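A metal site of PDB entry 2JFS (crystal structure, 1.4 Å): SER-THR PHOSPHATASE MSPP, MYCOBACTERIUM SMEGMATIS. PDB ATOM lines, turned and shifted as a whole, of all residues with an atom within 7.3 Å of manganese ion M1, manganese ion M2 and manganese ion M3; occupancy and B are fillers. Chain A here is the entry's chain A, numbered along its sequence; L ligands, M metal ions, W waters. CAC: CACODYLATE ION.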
ATOM      1  N   ARG A  18       9.990 -28.442  -9.564  1.00  0.00           N
ATOM      2  CA  ARG A  18      11.377 -27.970  -9.470  1.00  0.00           C
ATOM      3  C   ARG A  18      12.348 -29.144  -9.494  1.00  0.00           C
ATOM      4  O   ARG A  18      12.033 -30.204  -8.912  1.00  0.00           O
ATOM      5  CB  ARG A  18      11.589 -27.156  -8.182  1.00  0.00           C
ATOM      6  CG  ARG A  18      10.637 -25.942  -7.978  1.00  0.00           C
ATOM      7  CD  ARG A  18      10.941 -24.859  -8.964  1.00  0.00           C
ATOM      8  NE  ARG A  18      10.036 -23.709  -8.864  1.00  0.00           N
ATOM      9  CZ  ARG A  18      10.397 -22.484  -8.460  1.00  0.00           C
ATOM     10  NH1 ARG A  18      11.651 -22.267  -8.100  1.00  0.00           N
ATOM     11  NH2 ARG A  18       9.507 -21.480  -8.408  1.00  0.00           N
ATOM     12  N   ASN A  21      15.523 -28.861  -4.444  1.00  0.00           N
ATOM     13  CA  ASN A  21      14.956 -28.117  -3.343  1.00  0.00           C
ATOM     14  C   ASN A  21      15.993 -27.137  -2.817  1.00  0.00           C
ATOM     15  O   ASN A  21      17.043 -27.537  -2.254  1.00  0.00           O
ATOM     16  CB  ASN A  21      14.475 -29.055  -2.246  1.00  0.00           C
ATOM     17  CG  ASN A  21      13.643 -28.322  -1.179  1.00  0.00           C
ATOM     18  OD1 ASN A  21      13.541 -27.080  -1.166  1.00  0.00           O
ATOM     19  ND2 ASN A  21      13.028 -29.079  -0.290  1.00  0.00           N
ATOM     20  N   GLN A  22      15.723 -25.846  -3.027  1.00  0.00           N
ATOM     21  CA  GLN A  22      16.657 -24.798  -2.615  1.00  0.00           C
ATOM     22  C   GLN A  22      16.225 -24.067  -1.344  1.00  0.00           C
ATOM     23  O   GLN A  22      16.856 -23.081  -0.949  1.00  0.00           O
ATOM     24  CB  GLN A  22      16.931 -23.815  -3.741  1.00  0.00           C
ATOM     25  CG  GLN A  22      17.549 -24.492  -4.982  1.00  0.00           C
ATOM     26  CD  GLN A  22      17.967 -23.499  -6.021  1.00  0.00           C
ATOM     27  OE1 GLN A  22      17.312 -22.480  -6.228  1.00  0.00           O
ATOM     28  NE2 GLN A  22      19.083 -23.786  -6.693  1.00  0.00           N
ATOM     29  N   ASP A  23      15.133 -24.550  -0.736  1.00  0.00           N
ATOM     30  CA  ASP A  23      14.696 -24.056   0.605  1.00  0.00           C
ATOM     31  C   ASP A  23      15.524 -24.776   1.677  1.00  0.00           C
ATOM     32  O   ASP A  23      15.994 -25.926   1.484  1.00  0.00           O
ATOM     33  CB  ASP A  23      13.226 -24.404   0.924  1.00  0.00           C
ATOM     34  CG  ASP A  23      12.194 -23.581   0.156  1.00  0.00           C
ATOM     35  OD1 ASP A  23      12.518 -22.616  -0.585  1.00  0.00           O
ATOM     36  OD2 ASP A  23      11.002 -23.905   0.420  1.00  0.00           O
ATOM     37  N   ALA A  35      14.880 -20.313   4.981  1.00  0.00           N
ATOM     38  CA  ALA A  35      15.684 -19.603   3.985  1.00  0.00           C
ATOM     39  C   ALA A  35      15.330 -20.168   2.600  1.00  0.00           C
ATOM     40  O   ALA A  35      15.386 -21.383   2.414  1.00  0.00           O
ATOM     41  CB  ALA A  35      17.203 -19.763   4.285  1.00  0.00           C
ATOM     42  N   ASP A  36      14.924 -19.306   1.677  1.00  0.00           N
ATOM     43  CA  ASP A  36      14.539 -19.708   0.319  1.00  0.00           C
ATOM     44  C   ASP A  36      15.617 -19.277  -0.652  1.00  0.00           C
ATOM     45  O   ASP A  36      15.768 -18.095  -0.954  1.00  0.00           O
ATOM     46  CB  ASP A  36      13.177 -19.083  -0.012  1.00  0.00           C
ATOM     47  CG  ASP A  36      12.698 -19.458  -1.403  1.00  0.00           C
ATOM     48  OD1 ASP A  36      13.486 -20.056  -2.164  1.00  0.00           O
ATOM     49  OD2 ASP A  36      11.540 -19.088  -1.677  1.00  0.00           O
ATOM     50  N   GLY A  37      16.446 -20.227  -1.055  1.00  0.00           N
ATOM     51  CA  GLY A  37      17.549 -19.954  -1.955  1.00  0.00           C
ATOM     52  C   GLY A  37      17.121 -19.752  -3.406  1.00  0.00           C
ATOM     53  O   GLY A  37      16.101 -20.267  -3.869  1.00  0.00           O
ATOM     54  N   PHE A  38      17.937 -19.007  -4.153  1.00  0.00           N
ATOM     55  CA  PHE A  38      17.644 -18.776  -5.551  1.00  0.00           C
ATOM     56  C   PHE A  38      18.940 -18.758  -6.333  1.00  0.00           C
ATOM     57  O   PHE A  38      20.024 -18.494  -5.778  1.00  0.00           O
ATOM     58  CB  PHE A  38      16.850 -17.461  -5.784  1.00  0.00           C
ATOM     59  CG  PHE A  38      17.562 -16.209  -5.299  1.00  0.00           C
ATOM     60  CD1 PHE A  38      18.491 -15.568  -6.119  1.00  0.00           C
ATOM     61  CD2 PHE A  38      17.320 -15.717  -4.019  1.00  0.00           C
ATOM     62  CE1 PHE A  38      19.182 -14.378  -5.687  1.00  0.00           C
ATOM     63  CE2 PHE A  38      17.978 -14.543  -3.575  1.00  0.00           C
ATOM     64  CZ  PHE A  38      18.898 -13.900  -4.392  1.00  0.00           C
ATOM     65  N   GLY A  39      18.838 -18.988  -7.644  1.00  0.00           N
ATOM     66  CA  GLY A  39      20.019 -19.035  -8.492  1.00  0.00           C
ATOM     67  C   GLY A  39      20.570 -20.452  -8.628  1.00  0.00           C
ATOM     68  O   GLY A  39      20.018 -21.383  -7.999  1.00  0.00           O
ATOM     69  N   GLY A  42      21.429 -21.732  -5.331  1.00  0.00           N
ATOM     70  CA  GLY A  42      20.535 -21.306  -4.253  1.00  0.00           C
ATOM     71  C   GLY A  42      20.467 -22.289  -3.096  1.00  0.00           C
ATOM     72  O   GLY A  42      20.269 -21.871  -1.947  1.00  0.00           O
ATOM     73  N   HIS A  43      20.630 -23.580  -3.360  1.00  0.00           N
ATOM     74  CA  HIS A  43      20.571 -24.577  -2.258  1.00  0.00           C
ATOM     75  C   HIS A  43      21.797 -24.412  -1.373  1.00  0.00           C
ATOM     76  O   HIS A  43      21.704 -24.534  -0.147  1.00  0.00           O
ATOM     77  CB  HIS A  43      20.452 -26.008  -2.798  1.00  0.00           C
ATOM     78  CG  HIS A  43      21.412 -26.313  -3.919  1.00  0.00           C
ATOM     79  ND1 HIS A  43      21.455 -25.599  -5.101  1.00  0.00           N
ATOM     80  CD2 HIS A  43      22.360 -27.270  -4.018  1.00  0.00           C
ATOM     81  CE1 HIS A  43      22.402 -26.089  -5.877  1.00  0.00           C
ATOM     82  NE2 HIS A  43      22.969 -27.109  -5.254  1.00  0.00           N
ATOM     83  N   GLY A  89      21.647 -16.472  -4.118  1.00  0.00           N
ATOM     84  CA  GLY A  89      21.541 -15.906  -2.807  1.00  0.00           C
ATOM     85  C   GLY A  89      20.351 -16.558  -2.128  1.00  0.00           C
ATOM     86  O   GLY A  89      19.908 -17.643  -2.540  1.00  0.00           O
ATOM     87  N   THR A  90      19.825 -15.916  -1.092  1.00  0.00           N
ATOM     88  CA  THR A  90      18.704 -16.507  -0.350  1.00  0.00           C
ATOM     89  C   THR A  90      17.897 -15.462   0.415  1.00  0.00           C
ATOM     90  O   THR A  90      18.418 -14.385   0.780  1.00  0.00           O
ATOM     91  CB  THR A  90      19.231 -17.620   0.640  1.00  0.00           C
ATOM     92  OG1 THR A  90      18.132 -18.313   1.205  1.00  0.00           O
ATOM     93  CG2 THR A  90      20.124 -17.039   1.763  1.00  0.00           C
ATOM     94  N   THR A  91      16.640 -15.768   0.670  1.00  0.00           N
ATOM     95  CA  THR A  91      15.902 -15.042   1.698  1.00  0.00           C
ATOM     96  C   THR A  91      16.283 -15.622   3.071  1.00  0.00           C
ATOM     97  O   THR A  91      16.912 -16.688   3.176  1.00  0.00           O
ATOM     98  CB  THR A  91      14.373 -15.209   1.537  1.00  0.00           C
ATOM     99  OG1 THR A  91      14.028 -16.561   1.944  1.00  0.00           O
ATOM    100  CG2 THR A  91      13.974 -14.985   0.091  1.00  0.00           C
ATOM    101  N   ASP A 112      11.197 -12.618   0.912  1.00  0.00           N
ATOM    102  CA  ASP A 112       9.755 -12.846   0.789  1.00  0.00           C
ATOM    103  C   ASP A 112       9.262 -14.161   1.393  1.00  0.00           C
ATOM    104  O   ASP A 112       8.267 -14.723   0.910  1.00  0.00           O
ATOM    105  CB  ASP A 112       9.278 -12.744  -0.681  1.00  0.00           C
ATOM    106  CG  ASP A 112       9.867 -13.836  -1.569  1.00  0.00           C
ATOM    107  OD1 ASP A 112      10.693 -14.641  -1.078  1.00  0.00           O
ATOM    108  OD2 ASP A 112       9.497 -13.870  -2.778  1.00  0.00           O
ATOM    109  N   SER A 113       9.901 -14.584   2.485  1.00  0.00           N
ATOM    110  CA  SER A 113       9.457 -15.801   3.166  1.00  0.00           C
ATOM    111  C   SER A 113       8.684 -15.375   4.400  1.00  0.00           C
ATOM    112  O   SER A 113       9.277 -14.926   5.373  1.00  0.00           O
ATOM    113  CB  SER A 113      10.659 -16.676   3.596  1.00  0.00           C
ATOM    114  OG  SER A 113      11.426 -17.084   2.455  1.00  0.00           O
ATOM    115  N   ARG A 153       5.867 -10.303  -8.662  1.00  0.00           N
ATOM    116  CA  ARG A 153       5.690 -10.823  -7.307  1.00  0.00           C
ATOM    117  C   ARG A 153       6.966 -11.510  -6.816  1.00  0.00           C
ATOM    118  O   ARG A 153       7.310 -11.395  -5.637  1.00  0.00           O
ATOM    119  CB  ARG A 153       4.497 -11.778  -7.292  1.00  0.00           C
ATOM    120  CG  ARG A 153       4.219 -12.452  -5.973  1.00  0.00           C
ATOM    121  CD  ARG A 153       3.034 -13.379  -6.131  1.00  0.00           C
ATOM    122  NE  ARG A 153       2.809 -14.102  -4.875  1.00  0.00           N
ATOM    123  CZ  ARG A 153       1.775 -14.908  -4.632  1.00  0.00           C
ATOM    124  NH1 ARG A 153       0.851 -15.142  -5.570  1.00  0.00           N
ATOM    125  NH2 ARG A 153       1.676 -15.487  -3.444  1.00  0.00           N
ATOM    126  N   HIS A 154       7.680 -12.172  -7.710  1.00  0.00           N
ATOM    127  CA  HIS A 154       8.796 -13.034  -7.286  1.00  0.00           C
ATOM    128  C   HIS A 154      10.139 -12.373  -7.369  1.00  0.00           C
ATOM    129  O   HIS A 154      11.142 -13.021  -6.964  1.00  0.00           O
ATOM    130  CB  HIS A 154       8.742 -14.408  -8.008  1.00  0.00           C
ATOM    131  CG  HIS A 154       7.587 -15.241  -7.575  1.00  0.00           C
ATOM    132  ND1 HIS A 154       7.665 -16.130  -6.518  1.00  0.00           N
ATOM    133  CD2 HIS A 154       6.298 -15.265  -7.997  1.00  0.00           C
ATOM    134  CE1 HIS A 154       6.476 -16.682  -6.319  1.00  0.00           C
ATOM    135  NE2 HIS A 154       5.635 -16.181  -7.204  1.00  0.00           N
ATOM    136  N   LEU A 155      10.185 -11.088  -7.810  1.00  0.00           N
ATOM    137  CA  LEU A 155      11.415 -10.314  -7.944  1.00  0.00           C
ATOM    138  C   LEU A 155      11.807  -9.664  -6.627  1.00  0.00           C
ATOM    139  O   LEU A 155      11.158  -8.726  -6.169  1.00  0.00           O
ATOM    140  CB  LEU A 155      11.275  -9.244  -9.039  1.00  0.00           C
ATOM    141  CG  LEU A 155      12.512  -8.435  -9.412  1.00  0.00           C
ATOM    142  CD1 LEU A 155      13.642  -9.360  -9.841  1.00  0.00           C
ATOM    143  CD2 LEU A 155      12.223  -7.430 -10.519  1.00  0.00           C
ATOM    144  N   LEU A 156      12.877 -10.167  -6.008  1.00  0.00           N
ATOM    145  CA  LEU A 156      13.290  -9.645  -4.707  1.00  0.00           C
ATOM    146  C   LEU A 156      13.868  -8.231  -4.778  1.00  0.00           C
ATOM    147  O   LEU A 156      14.594  -7.877  -5.716  1.00  0.00           O
ATOM    148  CB  LEU A 156      14.349 -10.570  -4.071  1.00  0.00           C
ATOM    149  CG  LEU A 156      13.846 -11.966  -3.742  1.00  0.00           C
ATOM    150  CD1 LEU A 156      14.999 -12.801  -3.231  1.00  0.00           C
ATOM    151  CD2 LEU A 156      12.684 -11.995  -2.765  1.00  0.00           C
ATOM    152  N   SER A 185       8.323 -20.570   3.292  1.00  0.00           N
ATOM    153  CA  SER A 185       8.802 -20.009   2.026  1.00  0.00           C
ATOM    154  C   SER A 185       7.574 -19.582   1.195  1.00  0.00           C
ATOM    155  O   SER A 185       6.406 -19.970   1.477  1.00  0.00           O
ATOM    156  CB  SER A 185       9.668 -21.012   1.247  1.00  0.00           C
ATOM    157  OG  SER A 185       8.908 -22.185   0.910  1.00  0.00           O
ATOM    158  N   ASP A 186       7.827 -18.807   0.135  1.00  0.00           N
ATOM    159  CA  ASP A 186       6.728 -18.338  -0.693  1.00  0.00           C
ATOM    160  C   ASP A 186       6.029 -19.452  -1.467  1.00  0.00           C
ATOM    161  O   ASP A 186       4.957 -19.210  -1.994  1.00  0.00           O
ATOM    162  CB  ASP A 186       7.207 -17.225  -1.636  1.00  0.00           C
ATOM    163  CG  ASP A 186       8.213 -17.686  -2.655  1.00  0.00           C
ATOM    164  OD1 ASP A 186       8.778 -18.796  -2.581  1.00  0.00           O
ATOM    165  OD2 ASP A 186       8.426 -16.889  -3.600  1.00  0.00           O
ATOM    166  N   GLY A 187       6.604 -20.650  -1.490  1.00  0.00           N
ATOM    167  CA  GLY A 187       5.972 -21.741  -2.243  1.00  0.00           C
ATOM    168  C   GLY A 187       4.594 -22.100  -1.720  1.00  0.00           C
ATOM    169  O   GLY A 187       3.750 -22.576  -2.472  1.00  0.00           O
ATOM    170  N   LEU A 188       4.373 -21.908  -0.410  1.00  0.00           N
ATOM    171  CA  LEU A 188       3.085 -22.288   0.163  1.00  0.00           C
ATOM    172  C   LEU A 188       1.931 -21.531  -0.484  1.00  0.00           C
ATOM    173  O   LEU A 188       0.849 -22.098  -0.727  1.00  0.00           O
ATOM    174  CB  LEU A 188       3.095 -22.004   1.665  1.00  0.00           C
ATOM    175  CG  LEU A 188       1.802 -22.241   2.467  1.00  0.00           C
ATOM    176  CD1 LEU A 188       1.339 -23.702   2.285  1.00  0.00           C
ATOM    177  CD2 LEU A 188       1.990 -21.917   3.959  1.00  0.00           C
ATOM    178  N   ASP A 224       6.491 -24.586  -6.815  1.00  0.00           N
ATOM    179  CA  ASP A 224       7.727 -24.211  -6.120  1.00  0.00           C
ATOM    180  C   ASP A 224       8.010 -25.205  -5.006  1.00  0.00           C
ATOM    181  O   ASP A 224       7.132 -26.015  -4.628  1.00  0.00           O
ATOM    182  CB  ASP A 224       7.605 -22.780  -5.556  1.00  0.00           C
ATOM    183  CG  ASP A 224       8.956 -22.146  -5.121  1.00  0.00           C
ATOM    184  OD1 ASP A 224      10.064 -22.699  -5.353  1.00  0.00           O
ATOM    185  OD2 ASP A 224       8.807 -21.011  -4.573  1.00  0.00           O
ATOM    186  N   ASN A 225       9.240 -25.168  -4.482  1.00  0.00           N
ATOM    187  CA  ASN A 225       9.552 -25.778  -3.190  1.00  0.00           C
ATOM    188  C   ASN A 225       8.674 -25.139  -2.106  1.00  0.00           C
ATOM    189  O   ASN A 225       8.488 -23.919  -2.130  1.00  0.00           O
ATOM    190  CB  ASN A 225      11.019 -25.544  -2.791  1.00  0.00           C
ATOM    191  CG  ASN A 225      12.025 -25.875  -3.891  1.00  0.00           C
ATOM    192  OD1 ASN A 225      13.042 -25.202  -3.981  1.00  0.00           O
ATOM    193  ND2 ASN A 225      11.757 -26.911  -4.691  1.00  0.00           N
ATOM    194  N   THR A 226       8.183 -25.925  -1.157  1.00  0.00           N
ATOM    195  CA  THR A 226       7.471 -25.364  -0.015  1.00  0.00           C
ATOM    196  C   THR A 226       8.076 -25.846   1.287  1.00  0.00           C
ATOM    197  O   THR A 226       8.287 -27.053   1.464  1.00  0.00           O
ATOM    198  CB  THR A 226       5.988 -25.810  -0.060  1.00  0.00           C
ATOM    199  OG1 THR A 226       5.394 -25.224  -1.215  1.00  0.00           O
ATOM    200  CG2 THR A 226       5.209 -25.331   1.216  1.00  0.00           C
HETATM  201 AS   CAC L   1      12.711 -17.560  -4.646  1.00  0.00          AS
HETATM  202  O1  CAC L   1      11.008 -18.126  -4.597  1.00  0.00           O
HETATM  203  O2  CAC L   1      13.809 -18.862  -4.934  1.00  0.00           O
HETATM  204  C1  CAC L   1      13.048 -16.291  -6.074  1.00  0.00           C
HETATM  205  C2  CAC L   1      13.193 -16.602  -3.031  1.00  0.00           C
HETATM  206 MN    MN M   1      10.368 -19.898  -3.369  1.00  0.00          MN
HETATM  207 MN    MN M   2      13.978 -20.714  -4.061  1.00  0.00          MN
HETATM  208 MN    MN M   3       9.378 -17.027  -5.443  1.00  0.00          MN
HETATM  209  O   HOH W   1      10.368 -15.031  -4.913  1.00  0.00           O
HETATM  210  O   HOH W   2      10.420 -17.343  -7.381  1.00  0.00           O
HETATM  211  O   HOH W   3      13.723 -22.712  -3.072  1.00  0.00           O
HETATM  212  O   HOH W   4      10.304 -21.691  -2.070  1.00  0.00           O
HETATM  213  O   HOH W   5       8.163 -18.897  -5.804  1.00  0.00           O
HETATM  214  O   HOH W   6      14.728 -21.895  -5.921  1.00  0.00           O
HETATM  215  O   HOH W   7      11.815 -21.030  -4.743  1.00  0.00           O
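Manganese ion M1 is bound by OD1 of Asp 186, 2.1 Å away.
Manganese ion M1 is bound by OD2 of Asp 36, 2.2 Å away.
Water W4 binds manganese ion M1, 2.2 Å away.
Manganese ion M1 is bound by an oxygen (O1) of the ligand (2.2 Å).
OD2 of Asp 224 binds manganese ion M1 (2.3 Å).
Water W7 binds manganese ion M1, at 2.3 Å.
Manganese ion M1 has six donor atoms within binding distance.
Three residues have an atom within 4 Å of manganese ion M1: Asp 36, Asp 186 and Asp 224.
Water W3 bridges the side-chain amide oxygen of Asn 225 (2.7 Å) and the side-chain carboxylate of Asp 23 (2.8 Å).
Water W1 lies within hydrogen-bond range of the side-chain carboxylate of Asp 112 (2.6 Å) and the backbone carbonyl oxygen of His 154 (3.0 Å).
Of the 27 residues printed, 2 come within 4 Å of manganese ion M3.
The nearest printed residue that does not touch manganese ion M3 is Asp 224 (4.1 Å).
Manganese ion M3 is bound by the side-chain carboxylate (OD2) of Asp 186 (2.1 Å), an oxygen (O1) of the ligand (2.1 Å), a ring nitrogen (ND1) of His 154 (2.2 Å), water W2 (2.2 Å), water W5 (2.3 Å) and water W1 (2.3 Å).
Manganese ion M3 has six donor atoms within binding distance.
Two residues have an atom within 4 Å of manganese ion M2: Asp 36 and Gly 37.
Manganese ion M2 is bound by an oxygen (O2) of the ligand, 2.1 Å away.
The side-chain carboxylate (OD1) of Asp 36 is bound to manganese ion M2 (2.1 Å).
The backbone carbonyl oxygen (O) of Gly 37 binds manganese ion M2 (2.2 Å).
Manganese ion M2 is bound by water W3, at 2.2 Å.
Water W7 is bound to manganese ion M2 (2.3 Å).
Manganese ion M2 is bound by water W6, at 2.3 Å.
N of Asp 36 sits at hydrogen-bond distance from OG1 of Thr 91 (2.9 Å).
OD1 of Asp 224 lies within salt-bridge range of NH1 of Arg 18, at 3.2 Å.
OG1 of Thr 90 sits at hydrogen-bond distance from N of Gly 37.
O of Gln 22 lies within hydrogen-bond range of N of Gly 37.
The side-chain hydroxyl (OG1) of Thr 90 lies within hydrogen-bond range of the backbone carbonyl oxygen (O) of Asp 36 (3.2 Å).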
